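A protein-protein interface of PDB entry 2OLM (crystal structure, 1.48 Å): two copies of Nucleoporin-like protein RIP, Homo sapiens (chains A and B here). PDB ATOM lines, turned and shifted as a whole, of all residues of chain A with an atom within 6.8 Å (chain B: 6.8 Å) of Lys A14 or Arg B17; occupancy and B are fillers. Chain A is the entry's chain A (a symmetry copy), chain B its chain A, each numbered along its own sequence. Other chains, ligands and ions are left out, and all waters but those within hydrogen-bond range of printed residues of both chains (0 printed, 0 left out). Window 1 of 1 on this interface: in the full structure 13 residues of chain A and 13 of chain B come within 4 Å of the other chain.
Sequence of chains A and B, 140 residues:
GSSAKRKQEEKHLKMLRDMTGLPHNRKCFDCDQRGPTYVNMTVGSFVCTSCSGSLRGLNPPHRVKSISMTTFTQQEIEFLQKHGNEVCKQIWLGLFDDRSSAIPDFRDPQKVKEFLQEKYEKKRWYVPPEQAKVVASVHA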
ATOM      1  N   GLU A   9       7.377  10.198  -3.440  1.00  0.00           N
ATOM      2  CA  GLU A   9       6.251   9.309  -3.114  1.00  0.00           C
ATOM      3  C   GLU A   9       5.891   9.378  -1.636  1.00  0.00           C
ATOM      4  O   GLU A   9       4.724   9.486  -1.281  1.00  0.00           O
ATOM      5  CB  GLU A   9       6.529   7.853  -3.512  1.00  0.00           C
ATOM      6  CG  GLU A   9       6.480   7.654  -5.015  1.00  0.00           C
ATOM      7  CD  GLU A   9       6.802   6.241  -5.438  1.00  0.00           C
ATOM      8  OE1 GLU A   9       7.261   5.436  -4.601  1.00  0.00           O
ATOM      9  OE2 GLU A   9       6.604   5.935  -6.638  1.00  0.00           O
ATOM     10  N   GLU A  10       6.887   9.314  -0.745  1.00  0.00           N
ATOM     11  CA  GLU A  10       6.580   9.326   0.664  1.00  0.00           C
ATOM     12  C   GLU A  10       6.142  10.707   1.134  1.00  0.00           C
ATOM     13  O   GLU A  10       5.287  10.830   2.003  1.00  0.00           O
ATOM     14  CB  GLU A  10       7.782   8.841   1.478  1.00  0.00           C
ATOM     15  CG  GLU A  10       8.202   7.416   1.128  1.00  0.00           C
ATOM     16  CD  GLU A  10       7.098   6.396   1.248  1.00  0.00           C
ATOM     17  OE1 GLU A  10       6.453   6.337   2.297  1.00  0.00           O
ATOM     18  OE2 GLU A  10       6.834   5.669   0.264  1.00  0.00           O
ATOM     19  N   LYS A  11       6.680  11.754   0.521  1.00  0.00           N
ATOM     20  CA  LYS A  11       6.239  13.122   0.801  1.00  0.00           C
ATOM     21  C   LYS A  11       4.767  13.292   0.477  1.00  0.00           C
ATOM     22  O   LYS A  11       4.005  13.874   1.260  1.00  0.00           O
ATOM     23  CB  LYS A  11       7.071  14.128  -0.002  1.00  0.00           C
ATOM     24  CG  LYS A  11       6.747  15.592   0.292  1.00  0.00           C
ATOM     25  CD  LYS A  11       7.529  16.541  -0.630  1.00  0.00           C
ATOM     26  N   HIS A  12       4.370  12.741  -0.655  1.00  0.00           N
ATOM     27  CA  HIS A  12       2.962  12.845  -1.048  1.00  0.00           C
ATOM     28  C   HIS A  12       2.027  12.112  -0.080  1.00  0.00           C
ATOM     29  O   HIS A  12       0.915  12.576   0.248  1.00  0.00           O
ATOM     30  CB  HIS A  12       2.776  12.347  -2.471  1.00  0.00           C
ATOM     31  CG  HIS A  12       3.439  13.202  -3.502  1.00  0.00           C
ATOM     32  ND1 HIS A  12       3.897  12.691  -4.695  1.00  0.00           N
ATOM     33  CD2 HIS A  12       3.775  14.511  -3.502  1.00  0.00           C
ATOM     34  CE1 HIS A  12       4.470  13.651  -5.395  1.00  0.00           C
ATOM     35  NE2 HIS A  12       4.395  14.772  -4.707  1.00  0.00           N
ATOM     36  N   LEU A  13       2.489  10.959   0.420  1.00  0.00           N
ATOM     37  CA  LEU A  13       1.709  10.200   1.386  1.00  0.00           C
ATOM     38  C   LEU A  13       1.656  10.945   2.724  1.00  0.00           C
ATOM     39  O   LEU A  13       0.637  10.944   3.413  1.00  0.00           O
ATOM     40  CB  LEU A  13       2.303   8.810   1.586  1.00  0.00           C
ATOM     41  CG  LEU A  13       2.160   7.863   0.398  1.00  0.00           C
ATOM     42  CD1 LEU A  13       2.836   6.529   0.727  1.00  0.00           C
ATOM     43  CD2 LEU A  13       0.671   7.655   0.074  1.00  0.00           C
ATOM     44  N   LYS A  14       2.746  11.606   3.107  1.00  0.00           N
ATOM     45  CA  LYS A  14       2.700  12.424   4.325  1.00  0.00           C
ATOM     46  C   LYS A  14       1.646  13.556   4.179  1.00  0.00           C
ATOM     47  O   LYS A  14       0.806  13.795   5.079  1.00  0.00           O
ATOM     48  CB  LYS A  14       4.096  12.981   4.626  1.00  0.00           C
ATOM     49  CG  LYS A  14       4.130  13.869   5.872  1.00  0.00           C
ATOM     50  CD  LYS A  14       5.492  14.564   6.110  1.00  0.00           C
ATOM     51  CE  LYS A  14       5.373  15.576   7.265  1.00  0.00           C
ATOM     52  NZ  LYS A  14       6.571  16.507   7.430  1.00  0.00           N
ATOM     53  N   MET A  15       1.684  14.207   3.016  1.00  0.00           N
ATOM     54  CA  MET A  15       0.714  15.277   2.706  1.00  0.00           C
ATOM     55  C   MET A  15      -0.722  14.743   2.693  1.00  0.00           C
ATOM     56  O   MET A  15      -1.622  15.369   3.219  1.00  0.00           O
ATOM     57  CB  MET A  15       1.062  15.914   1.358  1.00  0.00           C
ATOM     58  CG  MET A  15       2.331  16.702   1.363  1.00  0.00           C
ATOM     59  SD  MET A  15       3.016  17.026  -0.293  1.00  0.00           S
ATOM     60  CE  MET A  15       2.146  18.532  -0.779  1.00  0.00           C
ATOM     61  N   LEU A  16      -0.906  13.572   2.133  1.00  0.00           N
ATOM     62  CA  LEU A  16      -2.201  12.901   2.095  1.00  0.00           C
ATOM     63  C   LEU A  16      -2.743  12.612   3.491  1.00  0.00           C
ATOM     64  O   LEU A  16      -3.915  12.870   3.817  1.00  0.00           O
ATOM     65  CB  LEU A  16      -2.063  11.611   1.269  1.00  0.00           C
ATOM     66  CG  LEU A  16      -3.313  10.792   1.075  1.00  0.00           C
ATOM     67  CD1 LEU A  16      -4.367  11.618   0.307  1.00  0.00           C
ATOM     68  CD2 LEU A  16      -2.948   9.510   0.314  1.00  0.00           C
ATOM     69  N   ARG A  17      -1.876  12.095   4.356  1.00  0.00           N
ATOM     70  CA  ARG A  17      -2.297  11.764   5.722  1.00  0.00           C
ATOM     71  C   ARG A  17      -2.508  12.993   6.627  1.00  0.00           C
ATOM     72  O   ARG A  17      -3.291  12.931   7.586  1.00  0.00           O
ATOM     73  CB  ARG A  17      -1.298  10.790   6.320  1.00  0.00           C
ATOM     74  CG  ARG A  17      -1.262   9.447   5.605  1.00  0.00           C
ATOM     75  CD  ARG A  17      -2.558   8.656   5.747  1.00  0.00           C
ATOM     76  NE  ARG A  17      -2.539   7.461   4.912  1.00  0.00           N
ATOM     77  CZ  ARG A  17      -3.614   6.721   4.669  1.00  0.00           C
ATOM     78  NH1 ARG A  17      -4.756   7.054   5.208  1.00  0.00           N
ATOM     79  NH2 ARG A  17      -3.543   5.665   3.907  1.00  0.00           N
ATOM     80  N   ASP A  18      -1.846  14.100   6.305  1.00  0.00           N
ATOM     81  CA  ASP A  18      -2.194  15.383   6.888  1.00  0.00           C
ATOM     82  C   ASP A  18      -3.667  15.687   6.572  1.00  0.00           C
ATOM     83  O   ASP A  18      -4.426  16.086   7.450  1.00  0.00           O
ATOM     84  CB  ASP A  18      -1.269  16.485   6.394  1.00  0.00           C
ATOM     85  CG  ASP A  18      -1.556  17.835   7.040  1.00  0.00           C
ATOM     86  OD1 ASP A  18      -1.071  18.082   8.172  1.00  0.00           O
ATOM     87  OD2 ASP A  18      -2.278  18.648   6.399  1.00  0.00           O
ATOM     88  N   MET A  19      -4.078  15.456   5.327  1.00  0.00           N
ATOM     89  CA  MET A  19      -5.443  15.756   4.929  1.00  0.00           C
ATOM     90  C   MET A  19      -6.426  14.757   5.461  1.00  0.00           C
ATOM     91  O   MET A  19      -7.519  15.138   5.896  1.00  0.00           O
ATOM     92  CB  MET A  19      -5.565  15.789   3.406  1.00  0.00           C
ATOM     93  CG  MET A  19      -5.005  17.062   2.794  1.00  0.00           C
ATOM     94  SD  MET A  19      -5.205  17.134   0.999  1.00  0.00           S
ATOM     95  CE  MET A  19      -3.818  16.111   0.483  1.00  0.00           C
ATOM     96  N   SER A  68      -5.081   4.315  -0.372  1.00  0.00           N
ATOM     97  CA  SER A  68      -3.905   3.506   0.027  1.00  0.00           C
ATOM     98  C   SER A  68      -3.106   2.954  -1.142  1.00  0.00           C
ATOM     99  O   SER A  68      -1.921   2.638  -0.971  1.00  0.00           O
ATOM    100  CB  SER A  68      -4.353   2.361   0.897  1.00  0.00           C
ATOM    101  OG  SER A  68      -5.175   1.509   0.174  1.00  0.00           O
ATOM    102  N   HIS B  12      -0.723   9.345  13.264  1.00  0.00           N
ATOM    103  CA  HIS B  12       0.376   8.378  13.333  1.00  0.00           C
ATOM    104  C   HIS B  12       0.913   8.000  11.949  1.00  0.00           C
ATOM    105  O   HIS B  12       2.132   7.834  11.732  1.00  0.00           O
ATOM    106  CB  HIS B  12      -0.058   7.146  14.108  1.00  0.00           C
ATOM    107  CG  HIS B  12      -0.322   7.403  15.556  1.00  0.00           C
ATOM    108  ND1 HIS B  12      -1.228   6.661  16.279  1.00  0.00           N
ATOM    109  CD2 HIS B  12       0.148   8.348  16.400  1.00  0.00           C
ATOM    110  CE1 HIS B  12      -1.292   7.124  17.512  1.00  0.00           C
ATOM    111  NE2 HIS B  12      -0.454   8.135  17.623  1.00  0.00           N
ATOM    112  N   LEU B  13       0.000   7.892  10.976  1.00  0.00           N
ATOM    113  CA  LEU B  13       0.398   7.586   9.610  1.00  0.00           C
ATOM    114  C   LEU B  13       1.144   8.776   8.998  1.00  0.00           C
ATOM    115  O   LEU B  13       2.102   8.608   8.246  1.00  0.00           O
ATOM    116  CB  LEU B  13      -0.818   7.238   8.759  1.00  0.00           C
ATOM    117  CG  LEU B  13      -1.489   5.909   9.094  1.00  0.00           C
ATOM    118  CD1 LEU B  13      -2.712   5.716   8.191  1.00  0.00           C
ATOM    119  CD2 LEU B  13      -0.487   4.758   8.908  1.00  0.00           C
ATOM    120  N   LYS B  14       0.728   9.998   9.321  1.00  0.00           N
ATOM    121  CA  LYS B  14       1.484  11.164   8.846  1.00  0.00           C
ATOM    122  C   LYS B  14       2.933  11.135   9.406  1.00  0.00           C
ATOM    123  O   LYS B  14       3.929  11.331   8.669  1.00  0.00           O
ATOM    124  CB  LYS B  14       0.748  12.451   9.237  1.00  0.00           C
ATOM    125  CG  LYS B  14       1.486  13.718   8.800  1.00  0.00           C
ATOM    126  CD  LYS B  14       0.842  15.028   9.313  1.00  0.00           C
ATOM    127  CE  LYS B  14       1.751  16.227   8.987  1.00  0.00           C
ATOM    128  NZ  LYS B  14       1.356  17.537   9.662  1.00  0.00           N
ATOM    129  N   MET B  15       3.024  10.844  10.705  1.00  0.00           N
ATOM    130  CA  MET B  15       4.336  10.731  11.373  1.00  0.00           C
ATOM    131  C   MET B  15       5.178   9.605  10.764  1.00  0.00           C
ATOM    132  O   MET B  15       6.361   9.769  10.533  1.00  0.00           O
ATOM    133  CB  MET B  15       4.133  10.497  12.873  1.00  0.00           C
ATOM    134  CG  MET B  15       3.566  11.671  13.603  1.00  0.00           C
ATOM    135  SD  MET B  15       2.853  11.265  15.228  1.00  0.00           S
ATOM    136  CE  MET B  15       4.294  11.355  16.313  1.00  0.00           C
ATOM    137  N   LEU B  16       4.546   8.495  10.468  1.00  0.00           N
ATOM    138  CA  LEU B  16       5.193   7.355   9.828  1.00  0.00           C
ATOM    139  C   LEU B  16       5.757   7.708   8.456  1.00  0.00           C
ATOM    140  O   LEU B  16       6.908   7.388   8.106  1.00  0.00           O
ATOM    141  CB  LEU B  16       4.180   6.201   9.737  1.00  0.00           C
ATOM    142  CG  LEU B  16       4.674   4.909   9.140  1.00  0.00           C
ATOM    143  CD1 LEU B  16       5.819   4.337  10.003  1.00  0.00           C
ATOM    144  CD2 LEU B  16       3.499   3.926   9.052  1.00  0.00           C
ATOM    145  N   ARG B  17       4.957   8.410   7.660  1.00  0.00           N
ATOM    146  CA  ARG B  17       5.395   8.790   6.312  1.00  0.00           C
ATOM    147  C   ARG B  17       6.448   9.913   6.289  1.00  0.00           C
ATOM    148  O   ARG B  17       7.241  10.003   5.341  1.00  0.00           O
ATOM    149  CB  ARG B  17       4.174   9.145   5.482  1.00  0.00           C
ATOM    150  CG  ARG B  17       3.237   7.969   5.253  1.00  0.00           C
ATOM    151  CD  ARG B  17       3.855   6.865   4.400  1.00  0.00           C
ATOM    152  NE  ARG B  17       2.989   5.694   4.348  1.00  0.00           N
ATOM    153  CZ  ARG B  17       3.378   4.517   3.872  1.00  0.00           C
ATOM    154  NH1 ARG B  17       4.591   4.383   3.408  1.00  0.00           N
ATOM    155  NH2 ARG B  17       2.564   3.498   3.856  1.00  0.00           N
ATOM    156  N   ASP B  18       6.477  10.735   7.334  1.00  0.00           N
ATOM    157  CA  ASP B  18       7.601  11.623   7.565  1.00  0.00           C
ATOM    158  C   ASP B  18       8.882  10.780   7.679  1.00  0.00           C
ATOM    159  O   ASP B  18       9.899  11.101   7.071  1.00  0.00           O
ATOM    160  CB  ASP B  18       7.381  12.488   8.797  1.00  0.00           C
ATOM    161  CG  ASP B  18       8.508  13.486   9.031  1.00  0.00           C
ATOM    162  OD1 ASP B  18       8.500  14.571   8.399  1.00  0.00           O
ATOM    163  OD2 ASP B  18       9.408  13.168   9.858  1.00  0.00           O
ATOM    164  N   MET B  19       8.816   9.678   8.425  1.00  0.00           N
ATOM    165  CA  MET B  19       9.991   8.847   8.623  1.00  0.00           C
ATOM    166  C   MET B  19      10.324   8.030   7.410  1.00  0.00           C
ATOM    167  O   MET B  19      11.503   7.890   7.066  1.00  0.00           O
ATOM    168  CB  MET B  19       9.784   7.896   9.802  1.00  0.00           C
ATOM    169  CG  MET B  19       9.926   8.584  11.149  1.00  0.00           C
ATOM    170  SD  MET B  19       9.747   7.452  12.547  1.00  0.00           S
ATOM    171  CE  MET B  19       7.954   7.340  12.637  1.00  0.00           C
ATOM    172  N   THR B  20       9.334   7.491   6.706  1.00  0.00           N
ATOM    173  CA  THR B  20       9.658   6.618   5.579  1.00  0.00           C
ATOM    174  C   THR B  20      10.317   7.358   4.421  1.00  0.00           C
ATOM    175  O   THR B  20      10.937   6.720   3.559  1.00  0.00           O
ATOM    176  CB  THR B  20       8.467   5.862   5.053  1.00  0.00           C
ATOM    177  OG1 THR B  20       7.446   6.821   4.743  1.00  0.00           O
ATOM    178  CG2 THR B  20       7.937   4.855   6.068  1.00  0.00           C
ATOM    179  N   GLY B  21      10.187   8.682   4.414  1.00  0.00           N
ATOM    180  CA  GLY B  21      10.828   9.506   3.382  1.00  0.00           C
ATOM    181  C   GLY B  21      12.253   9.951   3.706  1.00  0.00           C
ATOM    182  O   GLY B  21      12.939  10.479   2.821  1.00  0.00           O
ATOM    183  N   LEU B  22      12.717   9.743   4.942  1.00  0.00           N
ATOM    184  CA  LEU B  22      14.103  10.099   5.307  1.00  0.00           C
ATOM    185  C   LEU B  22      15.082   9.205   4.531  1.00  0.00           C
ATOM    186  O   LEU B  22      14.826   8.023   4.351  1.00  0.00           O
ATOM    187  CB  LEU B  22      14.322   9.954   6.805  1.00  0.00           C
ATOM    188  CG  LEU B  22      13.458  10.865   7.658  1.00  0.00           C
ATOM    189  CD1 LEU B  22      13.542  10.558   9.166  1.00  0.00           C
ATOM    190  CD2 LEU B  22      13.840  12.356   7.364  1.00  0.00           C
ATOM    191  N   PRO B  36      11.697  -0.528   2.060  1.00  0.00           N
ATOM    192  CA  PRO B  36      11.084  -1.233   3.179  1.00  0.00           C
ATOM    193  C   PRO B  36       9.572  -1.337   3.087  1.00  0.00           C
ATOM    194  O   PRO B  36       8.896  -0.437   2.594  1.00  0.00           O
ATOM    195  CB  PRO B  36      11.501  -0.424   4.397  1.00  0.00           C
ATOM    196  CG  PRO B  36      11.868   0.874   3.912  1.00  0.00           C
ATOM    197  CD  PRO B  36      12.223   0.773   2.459  1.00  0.00           C
ATOM    198  N   ILE B  67       4.246  -1.893   7.468  1.00  0.00           N
ATOM    199  CA  ILE B  67       4.119  -0.435   7.389  1.00  0.00           C
ATOM    200  C   ILE B  67       2.708   0.009   7.026  1.00  0.00           C
ATOM    201  O   ILE B  67       2.158   0.923   7.652  1.00  0.00           O
ATOM    202  CB  ILE B  67       5.161   0.158   6.422  1.00  0.00           C
ATOM    203  CG1 ILE B  67       6.583  -0.046   6.992  1.00  0.00           C
ATOM    204  CG2 ILE B  67       4.878   1.640   6.137  1.00  0.00           C
ATOM    205  CD1 ILE B  67       7.676   0.364   6.086  1.00  0.00           C
ATOM    206  N   SER B  68       2.124  -0.677   6.063  1.00  0.00           N
ATOM    207  CA  SER B  68       0.814  -0.244   5.524  1.00  0.00           C
ATOM    208  C   SER B  68      -0.383  -0.802   6.277  1.00  0.00           C
ATOM    209  O   SER B  68      -1.471  -0.215   6.207  1.00  0.00           O
ATOM    210  CB  SER B  68       0.709  -0.643   4.075  1.00  0.00           C
ATOM    211  OG  SER B  68       0.731  -2.025   3.960  1.00  0.00           O
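Gly B21 touches Glu A10.
Leu A13 touches Arg B17.
Lys A14 touches Lys B14 (CG to O, 3.8 Å).
Arg B17 touches Lys A14.
Leu B13 touches Arg A17.
Lys B14 touches Arg A17 (N to CB, 3.7 Å).
The backbone carbonyl oxygen of Leu B16 lies close to the side-chain hydroxyl of Thr B20 (3.5 Å).
The backbone carbonyl oxygen (O) of Arg B17 sits at hydrogen-bond distance from the side-chain hydroxyl (OG1) of Thr B20.
Leu A13 touches Arg B17, and with the chains exchanged Arg A17 touches Leu B13.
Lys B14 touches its own counterpart, Lys A14.
Lys A14 touches Arg B17, and with the chains exchanged Arg A17 touches Lys B14.
Lys A14 touches Asp B18, and with the chains exchanged Asp A18 touches Lys B14.
9 positions are printed for both chains.
Of the 10 pairs that touch across the chains among the printed residues, 7 have their exchanged pair printed and touching as well.
Hydrophobic or aromatic side chains of chain A within 4 Å of the printed part of chain B: Leu A13.
Printed residues of chain B that touch a printed residue of chain A: Leu B13, Lys B14, Arg B17, Asp B18, Thr B20 and Gly B21.
Among the printed residues, Asp or Glu carboxylates within 4 Å of a Lys or Arg side-chain nitrogen of the other chain: Glu A10 with Arg B17, Lys A14 with Asp B18 and Asp A18 with Lys B14.
OG1 of Thr B20 sits at hydrogen-bond distance from OE1 of Glu A10, at 2.7 Å.
The guanidinium group of Arg B17 lies within salt-bridge range of the side-chain carboxylate of Glu A10 (2.9 Å).
OD1 of Asp B18 lies within salt-bridge range of NZ of Lys A14, at 2.9 Å.
The side-chain amino group (NZ) of Lys B14 is in salt-bridge range of the side-chain carboxylate (OD1) of Asp A18.
Of chain B, only Lys B14 (3.8 Å), Arg B17 (3.7 Å) and Asp B18 (2.9 Å) come within 4 Å of Lys A14.
Printed residues of chain A within 4 Å of Leu B13: Arg A17 (3.7 Å).
Of the printed residues of chain B, Asp A18 touches Lys B14.
Of the printed residues of chain A, Lys B14 touches Lys A14, Arg A17 and Asp A18.
Of the printed residues of chain A, Asp B18 touches Lys A14.
Met A15 touches none of the printed residues of chain B.
The nearest residue of chain B that does not touch Lys A14 is Leu B13 (5.5 Å).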
